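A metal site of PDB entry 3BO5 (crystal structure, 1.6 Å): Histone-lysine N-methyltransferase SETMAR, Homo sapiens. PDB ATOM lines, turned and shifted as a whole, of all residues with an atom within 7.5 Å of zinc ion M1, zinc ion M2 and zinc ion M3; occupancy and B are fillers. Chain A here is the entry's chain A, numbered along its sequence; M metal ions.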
ATOM      1  N   PRO A  60     -14.284 -27.672  15.698  1.00  0.00           N
ATOM      2  CA  PRO A  60     -13.215 -26.659  15.700  1.00  0.00           C
ATOM      3  C   PRO A  60     -13.077 -25.832  16.975  1.00  0.00           C
ATOM      4  O   PRO A  60     -12.059 -25.142  17.138  1.00  0.00           O
ATOM      5  CB  PRO A  60     -13.591 -25.719  14.584  1.00  0.00           C
ATOM      6  CG  PRO A  60     -15.009 -25.910  14.307  1.00  0.00           C
ATOM      7  CD  PRO A  60     -15.371 -27.355  14.747  1.00  0.00           C
ATOM      8  N   GLY A  61     -14.071 -25.981  17.814  1.00  0.00           N
ATOM      9  CA  GLY A  61     -14.021 -25.311  19.145  1.00  0.00           C
ATOM     10  C   GLY A  61     -14.634 -23.919  19.157  1.00  0.00           C
ATOM     11  O   GLY A  61     -15.179 -23.410  18.146  1.00  0.00           O
ATOM     12  N   CYS A  62     -14.526 -23.272  20.332  1.00  0.00           N
ATOM     13  CA  CYS A  62     -15.070 -21.923  20.458  1.00  0.00           C
ATOM     14  C   CYS A  62     -13.973 -20.915  20.233  1.00  0.00           C
ATOM     15  O   CYS A  62     -12.770 -21.221  20.164  1.00  0.00           O
ATOM     16  CB  CYS A  62     -15.644 -21.764  21.851  1.00  0.00           C
ATOM     17  SG  CYS A  62     -14.421 -21.946  23.183  1.00  0.00           S
ATOM     18  N   ILE A  63     -14.447 -19.639  20.151  1.00  0.00           N
ATOM     19  CA  ILE A  63     -13.482 -18.593  19.849  1.00  0.00           C
ATOM     20  C   ILE A  63     -13.046 -17.790  21.058  1.00  0.00           C
ATOM     21  O   ILE A  63     -12.317 -16.821  20.908  1.00  0.00           O
ATOM     22  CB  ILE A  63     -14.020 -17.591  18.795  1.00  0.00           C
ATOM     23  CG1 ILE A  63     -15.218 -16.812  19.320  1.00  0.00           C
ATOM     24  CG2 ILE A  63     -14.345 -18.348  17.475  1.00  0.00           C
ATOM     25  CD1 ILE A  63     -15.728 -15.686  18.347  1.00  0.00           C
ATOM     26  N   CYS A  64     -13.401 -18.251  22.239  1.00  0.00           N
ATOM     27  CA  CYS A  64     -13.154 -17.466  23.441  1.00  0.00           C
ATOM     28  C   CYS A  64     -11.689 -17.527  23.725  1.00  0.00           C
ATOM     29  O   CYS A  64     -11.077 -18.615  23.656  1.00  0.00           O
ATOM     30  CB  CYS A  64     -13.869 -18.139  24.597  1.00  0.00           C
ATOM     31  SG  CYS A  64     -15.576 -18.503  24.199  1.00  0.00           S
ATOM     32  N   VAL A  65     -11.085 -16.363  23.909  1.00  0.00           N
ATOM     33  CA  VAL A  65      -9.696 -16.387  24.389  1.00  0.00           C
ATOM     34  C   VAL A  65      -9.469 -15.267  25.371  1.00  0.00           C
ATOM     35  O   VAL A  65      -8.789 -15.476  26.389  1.00  0.00           O
ATOM     36  CB  VAL A  65      -8.675 -16.310  23.260  1.00  0.00           C
ATOM     37  CG1 VAL A  65      -8.864 -15.019  22.415  1.00  0.00           C
ATOM     38  CG2 VAL A  65      -7.208 -16.525  23.889  1.00  0.00           C
ATOM     39  N   THR A  67     -11.742 -13.781  27.396  1.00  0.00           N
ATOM     40  CA  THR A  67     -12.525 -13.859  28.652  1.00  0.00           C
ATOM     41  C   THR A  67     -13.029 -15.277  28.764  1.00  0.00           C
ATOM     42  O   THR A  67     -13.007 -15.994  27.758  1.00  0.00           O
ATOM     43  CB  THR A  67     -13.775 -12.887  28.649  1.00  0.00           C
ATOM     44  OG1 THR A  67     -14.608 -13.206  27.529  1.00  0.00           O
ATOM     45  CG2 THR A  67     -13.313 -11.434  28.516  1.00  0.00           C
ATOM     46  N   PRO A  68     -13.477 -15.679  29.957  1.00  0.00           N
ATOM     47  CA  PRO A  68     -13.916 -17.068  30.107  1.00  0.00           C
ATOM     48  C   PRO A  68     -15.094 -17.433  29.203  1.00  0.00           C
ATOM     49  O   PRO A  68     -15.899 -16.608  28.745  1.00  0.00           O
ATOM     50  CB  PRO A  68     -14.364 -17.147  31.577  1.00  0.00           C
ATOM     51  CG  PRO A  68     -13.431 -16.086  32.264  1.00  0.00           C
ATOM     52  CD  PRO A  68     -13.416 -14.962  31.257  1.00  0.00           C
ATOM     53  N   CYS A  69     -15.198 -18.750  29.006  1.00  0.00           N
ATOM     54  CA  CYS A  69     -16.261 -19.268  28.255  1.00  0.00           C
ATOM     55  C   CYS A  69     -17.546 -19.130  29.086  1.00  0.00           C
ATOM     56  O   CYS A  69     -17.679 -19.703  30.185  1.00  0.00           O
ATOM     57  CB  CYS A  69     -15.976 -20.757  27.959  1.00  0.00           C
ATOM     58  SG  CYS A  69     -14.565 -20.912  26.887  1.00  0.00           S
ATOM     59  N   LEU A  70     -18.464 -18.423  28.499  1.00  0.00           N
ATOM     60  CA  LEU A  70     -19.787 -18.252  29.142  1.00  0.00           C
ATOM     61  C   LEU A  70     -20.901 -18.374  28.125  1.00  0.00           C
ATOM     62  O   LEU A  70     -20.735 -18.095  26.910  1.00  0.00           O
ATOM     63  CB  LEU A  70     -19.840 -16.923  29.893  1.00  0.00           C
ATOM     64  CG  LEU A  70     -18.975 -16.837  31.164  1.00  0.00           C
ATOM     65  CD1 LEU A  70     -18.760 -15.348  31.464  1.00  0.00           C
ATOM     66  CD2 LEU A  70     -19.596 -17.545  32.325  1.00  0.00           C
ATOM     67  N   THR A  73     -21.722 -16.310  24.554  1.00  0.00           N
ATOM     68  CA  THR A  73     -20.535 -15.889  23.791  1.00  0.00           C
ATOM     69  C   THR A  73     -19.642 -17.103  23.435  1.00  0.00           C
ATOM     70  O   THR A  73     -18.755 -17.022  22.603  1.00  0.00           O
ATOM     71  CB  THR A  73     -19.738 -14.811  24.514  1.00  0.00           C
ATOM     72  OG1 THR A  73     -19.412 -15.254  25.828  1.00  0.00           O
ATOM     73  CG2 THR A  73     -20.609 -13.560  24.719  1.00  0.00           C
ATOM     74  N   CYS A  74     -19.926 -18.236  24.053  1.00  0.00           N
ATOM     75  CA  CYS A  74     -19.116 -19.438  23.846  1.00  0.00           C
ATOM     76  C   CYS A  74     -19.902 -20.425  23.045  1.00  0.00           C
ATOM     77  O   CYS A  74     -20.989 -20.856  23.472  1.00  0.00           O
ATOM     78  CB  CYS A  74     -18.761 -20.053  25.190  1.00  0.00           C
ATOM     79  SG  CYS A  74     -17.828 -21.585  24.922  1.00  0.00           S
ATOM     80  N   SER A  75     -19.410 -20.724  21.841  1.00  0.00           N
ATOM     81  CA  SER A  75     -20.164 -21.668  20.963  1.00  0.00           C
ATOM     82  C   SER A  75     -20.176 -23.089  21.484  1.00  0.00           C
ATOM     83  O   SER A  75     -20.935 -23.946  21.033  1.00  0.00           O
ATOM     84  CB  SER A  75     -19.674 -21.636  19.507  1.00  0.00           C
ATOM     85  OG  SER A  75     -18.275 -21.846  19.409  1.00  0.00           O
ATOM     86  N   CYS A  76     -19.319 -23.364  22.458  1.00  0.00           N
ATOM     87  CA  CYS A  76     -19.398 -24.645  23.178  1.00  0.00           C
ATOM     88  C   CYS A  76     -20.505 -24.717  24.237  1.00  0.00           C
ATOM     89  O   CYS A  76     -20.747 -25.823  24.765  1.00  0.00           O
ATOM     90  CB  CYS A  76     -18.048 -24.997  23.851  1.00  0.00           C
ATOM     91  SG  CYS A  76     -16.723 -25.127  22.703  1.00  0.00           S
ATOM     92  N   LEU A  77     -21.119 -23.589  24.578  1.00  0.00           N
ATOM     93  CA  LEU A  77     -22.089 -23.492  25.644  1.00  0.00           C
ATOM     94  C   LEU A  77     -23.418 -23.007  25.123  1.00  0.00           C
ATOM     95  O   LEU A  77     -24.050 -22.152  25.760  1.00  0.00           O
ATOM     96  CB  LEU A  77     -21.624 -22.517  26.721  1.00  0.00           C
ATOM     97  CG  LEU A  77     -20.400 -23.009  27.479  1.00  0.00           C
ATOM     98  CD1 LEU A  77     -19.977 -22.040  28.603  1.00  0.00           C
ATOM     99  CD2 LEU A  77     -20.624 -24.368  28.065  1.00  0.00           C
ATOM    100  N   PHE A 103     -21.403 -30.340  24.977  1.00  0.00           N
ATOM    101  CA  PHE A 103     -20.078 -30.214  24.371  1.00  0.00           C
ATOM    102  C   PHE A 103     -19.147 -29.605  25.381  1.00  0.00           C
ATOM    103  O   PHE A 103     -19.468 -28.594  25.933  1.00  0.00           O
ATOM    104  CB  PHE A 103     -20.163 -29.292  23.145  1.00  0.00           C
ATOM    105  CG  PHE A 103     -20.869 -29.927  22.017  1.00  0.00           C
ATOM    106  CD1 PHE A 103     -20.143 -30.587  21.015  1.00  0.00           C
ATOM    107  CD2 PHE A 103     -22.274 -29.855  21.944  1.00  0.00           C
ATOM    108  CE1 PHE A 103     -20.804 -31.211  19.941  1.00  0.00           C
ATOM    109  CE2 PHE A 103     -22.949 -30.475  20.852  1.00  0.00           C
ATOM    110  CZ  PHE A 103     -22.215 -31.120  19.890  1.00  0.00           C
ATOM    111  N   GLU A 104     -18.027 -30.254  25.640  1.00  0.00           N
ATOM    112  CA  GLU A 104     -16.921 -29.608  26.402  1.00  0.00           C
ATOM    113  C   GLU A 104     -16.028 -28.785  25.471  1.00  0.00           C
ATOM    114  O   GLU A 104     -15.913 -29.074  24.262  1.00  0.00           O
ATOM    115  CB  GLU A 104     -16.054 -30.661  27.134  1.00  0.00           C
ATOM    116  CG  GLU A 104     -16.863 -31.301  28.227  1.00  0.00           C
ATOM    117  CD  GLU A 104     -16.005 -32.010  29.294  1.00  0.00           C
ATOM    118  OE1 GLU A 104     -14.737 -32.081  29.184  1.00  0.00           O
ATOM    119  OE2 GLU A 104     -16.697 -32.549  30.189  1.00  0.00           O
ATOM    120  N   CYS A 105     -15.315 -27.802  26.066  1.00  0.00           N
ATOM    121  CA  CYS A 105     -14.240 -27.168  25.308  1.00  0.00           C
ATOM    122  C   CYS A 105     -13.175 -28.249  25.044  1.00  0.00           C
ATOM    123  O   CYS A 105     -13.061 -29.216  25.771  1.00  0.00           O
ATOM    124  CB  CYS A 105     -13.726 -25.972  26.063  1.00  0.00           C
ATOM    125  SG  CYS A 105     -14.895 -24.683  26.035  1.00  0.00           S
ATOM    126  N   ASN A 106     -12.521 -28.126  23.871  1.00  0.00           N
ATOM    127  CA  ASN A 106     -11.680 -29.181  23.383  1.00  0.00           C
ATOM    128  C   ASN A 106     -10.263 -28.723  23.083  1.00  0.00           C
ATOM    129  O   ASN A 106      -9.856 -27.671  23.512  1.00  0.00           O
ATOM    130  CB  ASN A 106     -12.333 -29.913  22.216  1.00  0.00           C
ATOM    131  CG  ASN A 106     -12.417 -29.068  20.964  1.00  0.00           C
ATOM    132  OD1 ASN A 106     -11.669 -28.124  20.786  1.00  0.00           O
ATOM    133  ND2 ASN A 106     -13.299 -29.469  20.023  1.00  0.00           N
ATOM    134  N   LEU A 108      -8.932 -27.632  20.577  1.00  0.00           N
ATOM    135  CA  LEU A 108      -8.832 -26.477  19.715  1.00  0.00           C
ATOM    136  C   LEU A 108      -9.360 -25.185  20.306  1.00  0.00           C
ATOM    137  O   LEU A 108      -9.148 -24.061  19.707  1.00  0.00           O
ATOM    138  CB  LEU A 108      -9.515 -26.757  18.407  1.00  0.00           C
ATOM    139  CG  LEU A 108      -8.860 -27.943  17.693  1.00  0.00           C
ATOM    140  CD1 LEU A 108      -9.633 -27.979  16.381  1.00  0.00           C
ATOM    141  CD2 LEU A 108      -7.342 -27.799  17.481  1.00  0.00           C
ATOM    142  N   CYS A 109     -10.122 -25.269  21.399  1.00  0.00           N
ATOM    143  CA  CYS A 109     -10.624 -24.084  22.074  1.00  0.00           C
ATOM    144  C   CYS A 109      -9.399 -23.357  22.666  1.00  0.00           C
ATOM    145  O   CYS A 109      -8.581 -23.998  23.278  1.00  0.00           O
ATOM    146  CB  CYS A 109     -11.627 -24.513  23.183  1.00  0.00           C
ATOM    147  SG  CYS A 109     -13.113 -25.258  22.495  1.00  0.00           S
ATOM    148  N   ARG A 110      -9.400 -22.027  22.600  1.00  0.00           N
ATOM    149  CA  ARG A 110      -8.236 -21.340  23.131  1.00  0.00           C
ATOM    150  C   ARG A 110      -8.429 -20.905  24.543  1.00  0.00           C
ATOM    151  O   ARG A 110      -7.467 -20.392  25.139  1.00  0.00           O
ATOM    152  CB  ARG A 110      -7.883 -20.162  22.263  1.00  0.00           C
ATOM    153  CG  ARG A 110      -7.261 -20.657  20.981  1.00  0.00           C
ATOM    154  CD  ARG A 110      -7.662 -19.806  19.810  1.00  0.00           C
ATOM    155  NE  ARG A 110      -7.035 -18.524  19.949  1.00  0.00           N
ATOM    156  CZ  ARG A 110      -7.182 -17.520  19.100  1.00  0.00           C
ATOM    157  NH1 ARG A 110      -6.550 -16.364  19.341  1.00  0.00           N
ATOM    158  NH2 ARG A 110      -7.953 -17.668  18.028  1.00  0.00           N
ATOM    159  N   CYS A 111      -9.611 -21.176  25.121  1.00  0.00           N
ATOM    160  CA  CYS A 111      -9.730 -21.014  26.566  1.00  0.00           C
ATOM    161  C   CYS A 111      -8.695 -21.850  27.323  1.00  0.00           C
ATOM    162  O   CYS A 111      -8.188 -22.866  26.798  1.00  0.00           O
ATOM    163  CB  CYS A 111     -11.144 -21.356  27.057  1.00  0.00           C
ATOM    164  SG  CYS A 111     -11.540 -23.093  26.560  1.00  0.00           S
ATOM    165  N   SER A 112      -8.382 -21.483  28.554  1.00  0.00           N
ATOM    166  CA  SER A 112      -7.344 -22.199  29.276  1.00  0.00           C
ATOM    167  C   SER A 112      -7.795 -23.552  29.717  1.00  0.00           C
ATOM    168  O   SER A 112      -9.017 -23.879  29.685  1.00  0.00           O
ATOM    169  CB  SER A 112      -6.858 -21.450  30.508  1.00  0.00           C
ATOM    170  OG  SER A 112      -7.775 -21.625  31.559  1.00  0.00           O
ATOM    171  N   HIS A 114      -8.154 -24.385  32.505  1.00  0.00           N
ATOM    172  CA  HIS A 114      -8.995 -24.108  33.686  1.00  0.00           C
ATOM    173  C   HIS A 114     -10.442 -23.788  33.381  1.00  0.00           C
ATOM    174  O   HIS A 114     -11.276 -23.517  34.265  1.00  0.00           O
ATOM    175  CB  HIS A 114      -8.343 -23.057  34.555  1.00  0.00           C
ATOM    176  CG  HIS A 114      -6.946 -23.429  34.926  1.00  0.00           C
ATOM    177  ND1 HIS A 114      -5.833 -22.793  34.417  1.00  0.00           N
ATOM    178  CD2 HIS A 114      -6.475 -24.470  35.663  1.00  0.00           C
ATOM    179  CE1 HIS A 114      -4.739 -23.372  34.870  1.00  0.00           C
ATOM    180  NE2 HIS A 114      -5.097 -24.403  35.631  1.00  0.00           N
ATOM    181  N   CYS A 115     -10.763 -23.801  32.093  1.00  0.00           N
ATOM    182  CA  CYS A 115     -12.089 -23.452  31.701  1.00  0.00           C
ATOM    183  C   CYS A 115     -13.062 -24.392  32.438  1.00  0.00           C
ATOM    184  O   CYS A 115     -12.835 -25.601  32.498  1.00  0.00           O
ATOM    185  CB  CYS A 115     -12.241 -23.692  30.181  1.00  0.00           C
ATOM    186  SG  CYS A 115     -13.925 -23.440  29.556  1.00  0.00           S
ATOM    187  N   ARG A 116     -14.157 -23.819  32.950  1.00  0.00           N
ATOM    188  CA  ARG A 116     -15.183 -24.608  33.664  1.00  0.00           C
ATOM    189  C   ARG A 116     -15.905 -25.603  32.783  1.00  0.00           C
ATOM    190  O   ARG A 116     -16.567 -26.498  33.347  1.00  0.00           O
ATOM    191  CB  ARG A 116     -16.228 -23.735  34.362  1.00  0.00           C
ATOM    192  CG  ARG A 116     -15.566 -23.127  35.616  1.00  0.00           C
ATOM    193  CD  ARG A 116     -16.219 -21.808  35.999  1.00  0.00           C
ATOM    194  NE  ARG A 116     -17.589 -21.912  36.495  1.00  0.00           N
ATOM    195  CZ  ARG A 116     -18.258 -20.870  36.984  1.00  0.00           C
ATOM    196  NH1 ARG A 116     -19.492 -21.015  37.428  1.00  0.00           N
ATOM    197  NH2 ARG A 116     -17.671 -19.674  37.028  1.00  0.00           N
ATOM    198  N   ASN A 117     -15.764 -25.458  31.466  1.00  0.00           N
ATOM    199  CA  ASN A 117     -16.401 -26.416  30.563  1.00  0.00           C
ATOM    200  C   ASN A 117     -15.427 -27.499  30.103  1.00  0.00           C
ATOM    201  O   ASN A 117     -15.635 -28.067  29.020  1.00  0.00           O
ATOM    202  CB  ASN A 117     -17.044 -25.694  29.349  1.00  0.00           C
ATOM    203  CG  ASN A 117     -18.015 -26.542  28.625  1.00  0.00           C
ATOM    204  OD1 ASN A 117     -18.857 -27.176  29.254  1.00  0.00           O
ATOM    205  ND2 ASN A 117     -17.974 -26.485  27.294  1.00  0.00           N
ATOM    206  N   ARG A 118     -14.410 -27.784  30.931  1.00  0.00           N
ATOM    207  CA  ARG A 118     -13.501 -28.954  30.720  1.00  0.00           C
ATOM    208  C   ARG A 118     -13.600 -29.759  31.992  1.00  0.00           C
ATOM    209  O   ARG A 118     -13.122 -29.302  33.048  1.00  0.00           O
ATOM    210  CB  ARG A 118     -12.051 -28.491  30.493  1.00  0.00           C
ATOM    211  CG  ARG A 118     -11.911 -27.545  29.313  1.00  0.00           C
ATOM    212  CD  ARG A 118     -10.516 -27.035  29.280  1.00  0.00           C
ATOM    213  NE  ARG A 118     -10.214 -26.138  28.141  1.00  0.00           N
ATOM    214  CZ  ARG A 118      -9.896 -26.524  26.928  1.00  0.00           C
ATOM    215  NH1 ARG A 118      -9.970 -27.799  26.573  1.00  0.00           N
ATOM    216  NH2 ARG A 118      -9.558 -25.571  26.011  1.00  0.00           N
HETATM  217 ZN    ZN M   1     -13.713 -23.072  27.304  1.00  0.00          ZN
HETATM  218 ZN    ZN M   2     -14.864 -24.231  23.719  1.00  0.00          ZN
HETATM  219 ZN    ZN M   3     -15.713 -20.763  24.770  1.00  0.00          ZN
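Zinc ion M3 is bound by SG of Cys 74 (2.3 Å), SG of Cys 64 (2.3 Å), SG of Cys 62 (2.4 Å) and SG of Cys 69 (2.4 Å).
Zinc ion M3 has four donor atoms within binding distance.
Along chain A the residues within 4 Å of zinc ion M1 span positions 69 to 115.
The backbone NH of Cys 76 lies close to the side-chain sulfur of Cys 74.
The side-chain sulfur of Cys 115 lies close to the backbone NH of Asn 117, 3.3 Å away.
N of Cys 111 is in hydrogen-bond range of O of Cys 64 (3.3 Å).
The backbone carbonyl oxygen (O) of Cys 111 sits at hydrogen-bond distance from the guanidinium group (NH2) of Arg 118.
The backbone NH of Cys 105 sits at hydrogen-bond distance from the backbone carbonyl oxygen of Asn 117 (3.0 Å).
The guanidinium group (NH1) of Arg 118 lies within hydrogen-bond range of the backbone carbonyl oxygen (O) of Cys 105 (3.5 Å).
N of Cys 109 is in hydrogen-bond range of OD1 of Asn 106 (3.3 Å).
The backbone carbonyl oxygen (O) of Cys 109 is in hydrogen-bond range of the guanidinium group (NH2) of Arg 118.
Within 4 Å of zinc ion M2: Cys 62, Cys 76, Cys 105 and Cys 109.
SG of Cys 115 is bound to zinc ion M1 (2.3 Å).
SG of Cys 111 binds zinc ion M1, at 2.3 Å.
SG of Cys 69 binds zinc ion M1 (2.4 Å).
Zinc ion M1 is bound by SG of Cys 105 (2.4 Å).
SG of Cys 76 is bound to zinc ion M2, at 2.3 Å.
The side-chain sulfur (SG) of Cys 105 is bound to zinc ion M2, at 2.4 Å.
SG of Cys 109 binds zinc ion M2, 2.4 Å away.
SG of Cys 62 binds zinc ion M2, at 2.4 Å.
Zinc ion M2 has four donor atoms within binding distance.
Four residues have an atom within 4 Å of zinc ion M3: Cys 62, Cys 64, Cys 69 and Cys 74.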
